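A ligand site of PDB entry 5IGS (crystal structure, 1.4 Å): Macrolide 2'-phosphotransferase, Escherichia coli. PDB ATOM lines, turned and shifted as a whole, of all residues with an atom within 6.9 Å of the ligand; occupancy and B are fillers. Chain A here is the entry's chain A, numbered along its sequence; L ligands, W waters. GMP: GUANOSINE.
N7 of the ligand lies within hydrogen-bond range of OH of Tyr 94, at 2.6 Å. The side-chain carboxylate of Asp 219 sits at hydrogen-bond distance from an oxygen (O5') of the ligand, 2.7 Å away. The backbone carbonyl oxygen (O) of Asp 99 lies within hydrogen-bond range of a nitrogen (N2) of the ligand, at 2.8 Å. A nitrogen (N1) of the ligand is in hydrogen-bond range of the backbone carbonyl oxygen (O) of Leu 97, at 2.7 Å. The backbone NH (N) of Leu 97 is in hydrogen-bond range of an oxygen (O6) of the ligand.
The backbone carbonyl oxygen (O) of Tyr 94 sits at hydrogen-bond distance from the backbone NH (N) of Val 50, 2.8 Å away. NH1 of Arg 52 lies within salt-bridge range of OD1 of Asp 219 (3.9 Å). The backbone carbonyl oxygen (O) of Ile 38 sits at hydrogen-bond distance from the backbone NH (N) of Asn 30 (2.7 Å). The side-chain carboxylate (OD2) of Asp 219 sits at hydrogen-bond distance from a ring nitrogen (NE2) of His 205 (2.9 Å). O of Arg 48 lies within hydrogen-bond range of N of Met 96, at 2.8 Å. O of His 205 is in hydrogen-bond range of N of Ile 218 (2.9 Å).
Ile 38 touches the ligand (CG1 to C5', 3.96 Å). Val 50 touches the ligand (CG2 to N7, 3.7 Å). Arg 52 touches the ligand. CE of Met 96 touches C2 of the ligand, at 3.6 Å. O of Gly 204 touches O3' of the ligand, at 3.99 Å. His 205 touches the ligand. Leu 207 touches the ligand. Ile 218 touches the ligand (CD1 to C2', 3.6 Å). Hydrophobic or aromatic side chains within 4 Å of the ligand: Ile 38, Val 50, Tyr 94, Met 96, Leu 97, His 205, Leu 207 and Ile 218. 12 residues have an atom within 4 Å of the ligand: Ile 38, Val 50, Arg 52, Tyr 94, Met 96, Leu 97, Asp 99, Gly 204, His 205, Leu 207, Ile 218 and Asp 219. The nearest printed residue that does not touch the ligand is Thr 101 (4.1 Å).
Water W2 lies within hydrogen-bond range of an oxygen (O3') of the ligand (2.6 Å), a ring nitrogen (NE2) of His 205 (2.8 Å) and the side-chain carboxylate of Asp 219 (3.0 Å). Water W5 bridges O of Gly 204 (2.7 Å) and O2' of the ligand (2.8 Å). Water W3 bridges N2 of the ligand (2.9 Å) and N of Thr 101 (3.2 Å). Water W7 lies within hydrogen-bond range of the guanidinium group (NH1) of Arg 52 (2.7 Å), the side-chain hydroxyl (OH) of Tyr 94 (3.0 Å) and an oxygen (O5') of the ligand (3.0 Å). Water W6 bridges OH of Tyr 202 (2.4 Å) and O3' of the ligand (3.3 Å).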
ATOM      1  N   ASN A  30       5.022 -16.226   1.542  1.00  0.00           N
ATOM      2  CA  ASN A  30       5.966 -16.891   2.418  1.00  0.00           C
ATOM      3  C   ASN A  30       7.233 -16.046   2.478  1.00  0.00           C
ATOM      4  O   ASN A  30       7.991 -15.965   1.503  1.00  0.00           O
ATOM      5  CB  ASN A  30       6.273 -18.304   1.925  1.00  0.00           C
ATOM      6  CG  ASN A  30       7.193 -19.070   2.842  1.00  0.00           C
ATOM      7  OD1 ASN A  30       7.996 -18.476   3.555  1.00  0.00           O
ATOM      8  ND2 ASN A  30       7.084 -20.381   2.830  1.00  0.00           N
ATOM      9  N   ILE A  38       8.371 -15.736  -1.480  1.00  0.00           N
ATOM     10  CA  ILE A  38       7.614 -16.601  -2.378  1.00  0.00           C
ATOM     11  C   ILE A  38       6.161 -16.242  -2.218  1.00  0.00           C
ATOM     12  O   ILE A  38       5.603 -16.349  -1.125  1.00  0.00           O
ATOM     13  CB  ILE A  38       7.819 -18.099  -2.062  1.00  0.00           C
ATOM     14  CG1 ILE A  38       9.329 -18.421  -2.030  1.00  0.00           C
ATOM     15  CG2 ILE A  38       7.061 -18.993  -3.053  1.00  0.00           C
ATOM     16  CD1 ILE A  38       9.998 -18.344  -3.363  1.00  0.00           C
ATOM     17  N   ILE A  40       2.299 -16.874  -3.924  1.00  0.00           N
ATOM     18  CA  ILE A  40       1.458 -17.567  -4.888  1.00  0.00           C
ATOM     19  C   ILE A  40       0.257 -16.667  -5.100  1.00  0.00           C
ATOM     20  O   ILE A  40      -0.489 -16.364  -4.139  1.00  0.00           O
ATOM     21  CB  ILE A  40       1.064 -18.981  -4.411  1.00  0.00           C
ATOM     22  CG1 ILE A  40       2.332 -19.833  -4.269  1.00  0.00           C
ATOM     23  CG2 ILE A  40       0.115 -19.619  -5.420  1.00  0.00           C
ATOM     24  CD1 ILE A  40       2.077 -21.256  -3.798  1.00  0.00           C
ATOM     25  N   ARG A  48      -3.187 -19.539 -11.037  1.00  0.00           N
ATOM     26  CA  ARG A  48      -2.195 -19.169 -10.040  1.00  0.00           C
ATOM     27  C   ARG A  48      -0.786 -19.184 -10.612  1.00  0.00           C
ATOM     28  O   ARG A  48      -0.438 -20.071 -11.394  1.00  0.00           O
ATOM     29  CB  ARG A  48      -2.286 -20.077  -8.846  1.00  0.00           C
ATOM     30  CG  ARG A  48      -3.611 -19.895  -8.099  1.00  0.00           C
ATOM     31  CD  ARG A  48      -3.461 -20.211  -6.655  1.00  0.00           C
ATOM     32  NE  ARG A  48      -3.194 -21.625  -6.463  1.00  0.00           N
ATOM     33  CZ  ARG A  48      -2.877 -22.183  -5.293  1.00  0.00           C
ATOM     34  NH1 ARG A  48      -2.793 -21.456  -4.180  1.00  0.00           N
ATOM     35  NH2 ARG A  48      -2.648 -23.492  -5.239  1.00  0.00           N
ATOM     36  N   VAL A  50       3.443 -18.554  -9.312  1.00  0.00           N
ATOM     37  CA  VAL A  50       4.415 -18.401  -8.241  1.00  0.00           C
ATOM     38  C   VAL A  50       5.327 -17.236  -8.586  1.00  0.00           C
ATOM     39  O   VAL A  50       5.895 -17.192  -9.677  1.00  0.00           O
ATOM     40  CB  VAL A  50       5.268 -19.676  -8.109  1.00  0.00           C
ATOM     41  CG1 VAL A  50       6.292 -19.539  -7.012  1.00  0.00           C
ATOM     42  CG2 VAL A  50       4.355 -20.862  -7.861  1.00  0.00           C
ATOM     43  N   ARG A  52       8.635 -15.624  -7.393  1.00  0.00           N
ATOM     44  CA  ARG A  52       9.851 -15.935  -6.683  1.00  0.00           C
ATOM     45  C   ARG A  52      10.692 -14.660  -6.727  1.00  0.00           C
ATOM     46  O   ARG A  52      11.252 -14.315  -7.764  1.00  0.00           O
ATOM     47  CB  ARG A  52      10.503 -17.122  -7.398  1.00  0.00           C
ATOM     48  CG  ARG A  52      11.827 -17.556  -6.922  1.00  0.00           C
ATOM     49  CD  ARG A  52      12.212 -18.844  -7.673  1.00  0.00           C
ATOM     50  NE  ARG A  52      13.430 -19.409  -7.131  1.00  0.00           N
ATOM     51  CZ  ARG A  52      13.484 -20.103  -6.001  1.00  0.00           C
ATOM     52  NH1 ARG A  52      12.382 -20.362  -5.313  1.00  0.00           N
ATOM     53  NH2 ARG A  52      14.657 -20.542  -5.566  1.00  0.00           N
ATOM     54  N   PRO A  82       9.312 -25.981 -13.188  1.00  0.00           N
ATOM     55  CA  PRO A  82       8.791 -24.604 -13.339  1.00  0.00           C
ATOM     56  C   PRO A  82       9.133 -24.018 -14.709  1.00  0.00           C
ATOM     57  O   PRO A  82      10.264 -24.177 -15.220  1.00  0.00           O
ATOM     58  CB  PRO A  82       9.496 -23.859 -12.199  1.00  0.00           C
ATOM     59  CG  PRO A  82       9.728 -24.902 -11.144  1.00  0.00           C
ATOM     60  CD  PRO A  82      10.086 -26.144 -11.953  1.00  0.00           C
ATOM     61  N   TYR A  94       6.394 -18.097 -12.604  1.00  0.00           N
ATOM     62  CA  TYR A  94       5.983 -19.259 -13.387  1.00  0.00           C
ATOM     63  C   TYR A  94       4.573 -19.632 -13.010  1.00  0.00           C
ATOM     64  O   TYR A  94       4.159 -19.446 -11.866  1.00  0.00           O
ATOM     65  CB  TYR A  94       6.950 -20.425 -13.191  1.00  0.00           C
ATOM     66  CG  TYR A  94       7.239 -20.899 -11.791  1.00  0.00           C
ATOM     67  CD1 TYR A  94       8.289 -20.376 -11.061  1.00  0.00           C
ATOM     68  CD2 TYR A  94       6.514 -21.939 -11.217  1.00  0.00           C
ATOM     69  CE1 TYR A  94       8.607 -20.824  -9.809  1.00  0.00           C
ATOM     70  CE2 TYR A  94       6.835 -22.413  -9.947  1.00  0.00           C
ATOM     71  CZ  TYR A  94       7.902 -21.875  -9.265  1.00  0.00           C
ATOM     72  OH  TYR A  94       8.209 -22.360  -7.997  1.00  0.00           O
ATOM     73  N   PRO A  95       3.843 -20.223 -13.966  1.00  0.00           N
ATOM     74  CA  PRO A  95       2.522 -20.722 -13.608  1.00  0.00           C
ATOM     75  C   PRO A  95       2.688 -21.798 -12.535  1.00  0.00           C
ATOM     76  O   PRO A  95       3.550 -22.648 -12.622  1.00  0.00           O
ATOM     77  CB  PRO A  95       1.986 -21.334 -14.927  1.00  0.00           C
ATOM     78  CG  PRO A  95       2.858 -20.822 -15.980  1.00  0.00           C
ATOM     79  CD  PRO A  95       4.160 -20.417 -15.383  1.00  0.00           C
ATOM     80  N   MET A  96       1.853 -21.754 -11.513  1.00  0.00           N
ATOM     81  CA  MET A  96       1.962 -22.739 -10.463  1.00  0.00           C
ATOM     82  C   MET A  96       1.735 -24.116 -11.030  1.00  0.00           C
ATOM     83  O   MET A  96       0.853 -24.333 -11.861  1.00  0.00           O
ATOM     84  CB  MET A  96       0.950 -22.491  -9.323  1.00  0.00           C
ATOM     85  CG  MET A  96       1.253 -23.359  -8.102  1.00  0.00           C
ATOM     86  SD  MET A  96       0.031 -23.167  -6.811  1.00  0.00           S
ATOM     87  CE  MET A  96       0.631 -24.382  -5.643  1.00  0.00           C
ATOM     88  N   LEU A  97       2.552 -25.051 -10.565  1.00  0.00           N
ATOM     89  CA  LEU A  97       2.327 -26.476 -10.821  1.00  0.00           C
ATOM     90  C   LEU A  97       1.414 -26.928  -9.685  1.00  0.00           C
ATOM     91  O   LEU A  97       1.817 -27.021  -8.521  1.00  0.00           O
ATOM     92  CB  LEU A  97       3.661 -27.239 -10.851  1.00  0.00           C
ATOM     93  CG  LEU A  97       4.636 -26.779 -11.950  1.00  0.00           C
ATOM     94  CD1 LEU A  97       6.015 -27.407 -11.777  1.00  0.00           C
ATOM     95  CD2 LEU A  97       4.070 -27.061 -13.328  1.00  0.00           C
ATOM     96  N   GLU A  98       0.147 -27.130 -10.002  1.00  0.00           N
ATOM     97  CA  GLU A  98      -0.835 -27.229  -8.925  1.00  0.00           C
ATOM     98  C   GLU A  98      -0.799 -28.519  -8.118  1.00  0.00           C
ATOM     99  O   GLU A  98      -1.347 -28.591  -7.017  1.00  0.00           O
ATOM    100  CB  GLU A  98      -2.240 -26.951  -9.442  1.00  0.00           C
ATOM    101  CG  GLU A  98      -2.433 -25.500  -9.865  1.00  0.00           C
ATOM    102  CD  GLU A  98      -2.618 -24.564  -8.672  1.00  0.00           C
ATOM    103  OE1 GLU A  98      -2.557 -25.050  -7.514  1.00  0.00           O
ATOM    104  OE2 GLU A  98      -2.808 -23.348  -8.878  1.00  0.00           O
ATOM    105  N   ASP A  99      -0.150 -29.551  -8.646  1.00  0.00           N
ATOM    106  CA  ASP A  99      -0.016 -30.789  -7.889  1.00  0.00           C
ATOM    107  C   ASP A  99       0.698 -30.531  -6.564  1.00  0.00           C
ATOM    108  O   ASP A  99       1.632 -29.711  -6.473  1.00  0.00           O
ATOM    109  CB  ASP A  99       0.774 -31.837  -8.676  1.00  0.00           C
ATOM    110  CG  ASP A  99      -0.039 -32.517  -9.761  1.00  0.00           C
ATOM    111  OD1 ASP A  99      -1.247 -32.245  -9.866  1.00  0.00           O
ATOM    112  OD2 ASP A  99       0.540 -33.328 -10.527  1.00  0.00           O
ATOM    113  N   SER A 100       0.303 -31.257  -5.541  1.00  0.00           N
ATOM    114  CA  SER A 100       0.892 -31.121  -4.223  1.00  0.00           C
ATOM    115  C   SER A 100       2.348 -31.530  -4.175  1.00  0.00           C
ATOM    116  O   SER A 100       2.755 -32.439  -4.886  1.00  0.00           O
ATOM    117  CB  SER A 100       0.134 -32.012  -3.252  1.00  0.00           C
ATOM    118  OG  SER A 100       0.574 -31.884  -1.918  1.00  0.00           O
ATOM    119  N   THR A 101       3.106 -30.893  -3.303  1.00  0.00           N
ATOM    120  CA  THR A 101       4.378 -31.460  -2.890  1.00  0.00           C
ATOM    121  C   THR A 101       4.146 -32.788  -2.149  1.00  0.00           C
ATOM    122  O   THR A 101       3.051 -33.040  -1.604  1.00  0.00           O
ATOM    123  CB  THR A 101       5.155 -30.454  -2.009  1.00  0.00           C
ATOM    124  OG1 THR A 101       4.275 -29.936  -0.989  1.00  0.00           O
ATOM    125  CG2 THR A 101       5.623 -29.277  -2.854  1.00  0.00           C
ATOM    126  N   MET A 103       5.530 -33.708   0.541  1.00  0.00           N
ATOM    127  CA  MET A 103       5.456 -33.372   1.949  1.00  0.00           C
ATOM    128  C   MET A 103       4.719 -32.052   2.044  1.00  0.00           C
ATOM    129  O   MET A 103       5.021 -31.117   1.304  1.00  0.00           O
ATOM    130  CB  MET A 103       6.846 -33.231   2.557  1.00  0.00           C
ATOM    131  CG  MET A 103       6.813 -32.697   4.001  1.00  0.00           C
ATOM    132  SD  MET A 103       8.421 -32.258   4.624  1.00  0.00           S
ATOM    133  CE  MET A 103       8.736 -30.820   3.615  1.00  0.00           C
ATOM    134  N   ILE A 105       3.831 -28.990   4.655  1.00  0.00           N
ATOM    135  CA  ILE A 105       4.260 -28.410   5.920  1.00  0.00           C
ATOM    136  C   ILE A 105       3.829 -26.958   5.922  1.00  0.00           C
ATOM    137  O   ILE A 105       3.865 -26.283   4.880  1.00  0.00           O
ATOM    138  CB  ILE A 105       5.778 -28.561   6.128  1.00  0.00           C
ATOM    139  CG1 ILE A 105       6.181 -28.146   7.534  1.00  0.00           C
ATOM    140  CG2 ILE A 105       6.571 -27.771   5.078  1.00  0.00           C
ATOM    141  CD1 ILE A 105       7.567 -28.589   7.925  1.00  0.00           C
ATOM    142  N   TYR A 202      14.276 -33.689  -2.170  1.00  0.00           N
ATOM    143  CA  TYR A 202      13.645 -34.396  -1.061  1.00  0.00           C
ATOM    144  C   TYR A 202      12.156 -34.247  -1.305  1.00  0.00           C
ATOM    145  O   TYR A 202      11.730 -33.550  -2.222  1.00  0.00           O
ATOM    146  CB  TYR A 202      14.064 -33.842   0.320  1.00  0.00           C
ATOM    147  CG  TYR A 202      13.408 -32.587   0.786  1.00  0.00           C
ATOM    148  CD1 TYR A 202      13.596 -31.379   0.124  1.00  0.00           C
ATOM    149  CD2 TYR A 202      12.629 -32.588   1.909  1.00  0.00           C
ATOM    150  CE1 TYR A 202      13.017 -30.216   0.580  1.00  0.00           C
ATOM    151  CE2 TYR A 202      12.035 -31.455   2.369  1.00  0.00           C
ATOM    152  CZ  TYR A 202      12.249 -30.280   1.704  1.00  0.00           C
ATOM    153  OH  TYR A 202      11.640 -29.152   2.208  1.00  0.00           O
ATOM    154  N   GLY A 204       9.874 -32.514  -0.102  1.00  0.00           N
ATOM    155  CA  GLY A 204       9.340 -31.160  -0.194  1.00  0.00           C
ATOM    156  C   GLY A 204       9.497 -30.485  -1.546  1.00  0.00           C
ATOM    157  O   GLY A 204       8.867 -29.459  -1.795  1.00  0.00           O
ATOM    158  N   HIS A 205      10.355 -31.039  -2.419  1.00  0.00           N
ATOM    159  CA  HIS A 205      10.596 -30.462  -3.737  1.00  0.00           C
ATOM    160  C   HIS A 205      10.151 -31.384  -4.860  1.00  0.00           C
ATOM    161  O   HIS A 205      10.462 -31.140  -6.023  1.00  0.00           O
ATOM    162  CB  HIS A 205      12.068 -30.120  -3.904  1.00  0.00           C
ATOM    163  CG  HIS A 205      12.500 -28.984  -3.033  1.00  0.00           C
ATOM    164  ND1 HIS A 205      13.827 -28.728  -2.703  1.00  0.00           N
ATOM    165  CD2 HIS A 205      11.780 -28.030  -2.402  1.00  0.00           C
ATOM    166  CE1 HIS A 205      13.893 -27.667  -1.932  1.00  0.00           C
ATOM    167  NE2 HIS A 205      12.665 -27.230  -1.719  1.00  0.00           N
ATOM    168  N   LEU A 207       6.715 -33.028  -6.671  1.00  0.00           N
ATOM    169  CA  LEU A 207       5.280 -32.898  -6.832  1.00  0.00           C
ATOM    170  C   LEU A 207       4.703 -34.243  -7.228  1.00  0.00           C
ATOM    171  O   LEU A 207       5.325 -34.994  -7.997  1.00  0.00           O
ATOM    172  CB  LEU A 207       4.910 -31.878  -7.916  1.00  0.00           C
ATOM    173  CG  LEU A 207       5.545 -30.498  -7.765  1.00  0.00           C
ATOM    174  CD1 LEU A 207       4.978 -29.518  -8.776  1.00  0.00           C
ATOM    175  CD2 LEU A 207       5.360 -29.964  -6.316  1.00  0.00           C
ATOM    176  N   ILE A 218      10.524 -29.193  -8.184  1.00  0.00           N
ATOM    177  CA  ILE A 218      10.667 -27.755  -8.099  1.00  0.00           C
ATOM    178  C   ILE A 218      11.976 -27.399  -7.388  1.00  0.00           C
ATOM    179  O   ILE A 218      12.662 -28.278  -6.866  1.00  0.00           O
ATOM    180  CB  ILE A 218       9.464 -27.107  -7.352  1.00  0.00           C
ATOM    181  CG1 ILE A 218       9.371 -27.684  -5.945  1.00  0.00           C
ATOM    182  CG2 ILE A 218       8.172 -27.329  -8.133  1.00  0.00           C
ATOM    183  CD1 ILE A 218       8.330 -27.003  -5.067  1.00  0.00           C
ATOM    184  N   ASP A 219      12.299 -26.111  -7.381  1.00  0.00           N
ATOM    185  CA  ASP A 219      13.415 -25.580  -6.582  1.00  0.00           C
ATOM    186  C   ASP A 219      14.761 -26.158  -7.051  1.00  0.00           C
ATOM    187  O   ASP A 219      15.440 -26.888  -6.327  1.00  0.00           O
ATOM    188  CB  ASP A 219      13.185 -25.796  -5.088  1.00  0.00           C
ATOM    189  CG  ASP A 219      12.119 -24.873  -4.476  1.00  0.00           C
ATOM    190  OD1 ASP A 219      11.395 -24.160  -5.196  1.00  0.00           O
ATOM    191  OD2 ASP A 219      11.990 -24.860  -3.235  1.00  0.00           O
HETATM  192  O5' GMP L   1       9.724 -22.549  -3.747  1.00  0.00           O
HETATM  193  C5' GMP L   1       9.337 -22.368  -2.384  1.00  0.00           C
HETATM  194  C4' GMP L   1       8.252 -23.321  -1.892  1.00  0.00           C
HETATM  195  O4' GMP L   1       6.951 -22.937  -2.421  1.00  0.00           O
HETATM  196  C3' GMP L   1       8.399 -24.793  -2.267  1.00  0.00           C
HETATM  197  O3' GMP L   1       9.237 -25.512  -1.382  1.00  0.00           O
HETATM  198  C2' GMP L   1       6.954 -25.296  -2.273  1.00  0.00           C
HETATM  199  O2' GMP L   1       6.489 -25.545  -0.953  1.00  0.00           O
HETATM  200  C1' GMP L   1       6.215 -24.083  -2.810  1.00  0.00           C
HETATM  201  N9  GMP L   1       6.135 -24.076  -4.290  1.00  0.00           N
HETATM  202  C8  GMP L   1       6.853 -23.269  -5.136  1.00  0.00           C
HETATM  203  N7  GMP L   1       6.512 -23.550  -6.405  1.00  0.00           N
HETATM  204  C5  GMP L   1       5.510 -24.510  -6.387  1.00  0.00           C
HETATM  205  C6  GMP L   1       4.748 -25.176  -7.386  1.00  0.00           C
HETATM  206  O6  GMP L   1       4.852 -24.883  -8.693  1.00  0.00           O
HETATM  207  N1  GMP L   1       3.822 -26.104  -7.024  1.00  0.00           N
HETATM  208  C2  GMP L   1       3.629 -26.435  -5.651  1.00  0.00           C
HETATM  209  N2  GMP L   1       2.670 -27.400  -5.377  1.00  0.00           N
HETATM  210  N3  GMP L   1       4.336 -25.794  -4.641  1.00  0.00           N
HETATM  211  C4  GMP L   1       5.263 -24.863  -5.028  1.00  0.00           C
HETATM  212  O   HOH W   1       3.379 -25.963  -2.028  1.00  0.00           O
HETATM  213  O   HOH W   2      11.604 -25.146  -0.266  1.00  0.00           O
HETATM  214  O   HOH W   3       1.856 -28.045  -2.683  1.00  0.00           O
HETATM  215  O   HOH W   4       5.559 -21.083  -0.557  1.00  0.00           O
HETATM  216  O   HOH W   5       7.690 -27.841   0.057  1.00  0.00           O
HETATM  217  O   HOH W   6      10.484 -27.320   1.070  1.00  0.00           O
HETATM  218  O   HOH W   7       9.852 -20.652  -6.120  1.00  0.00           O
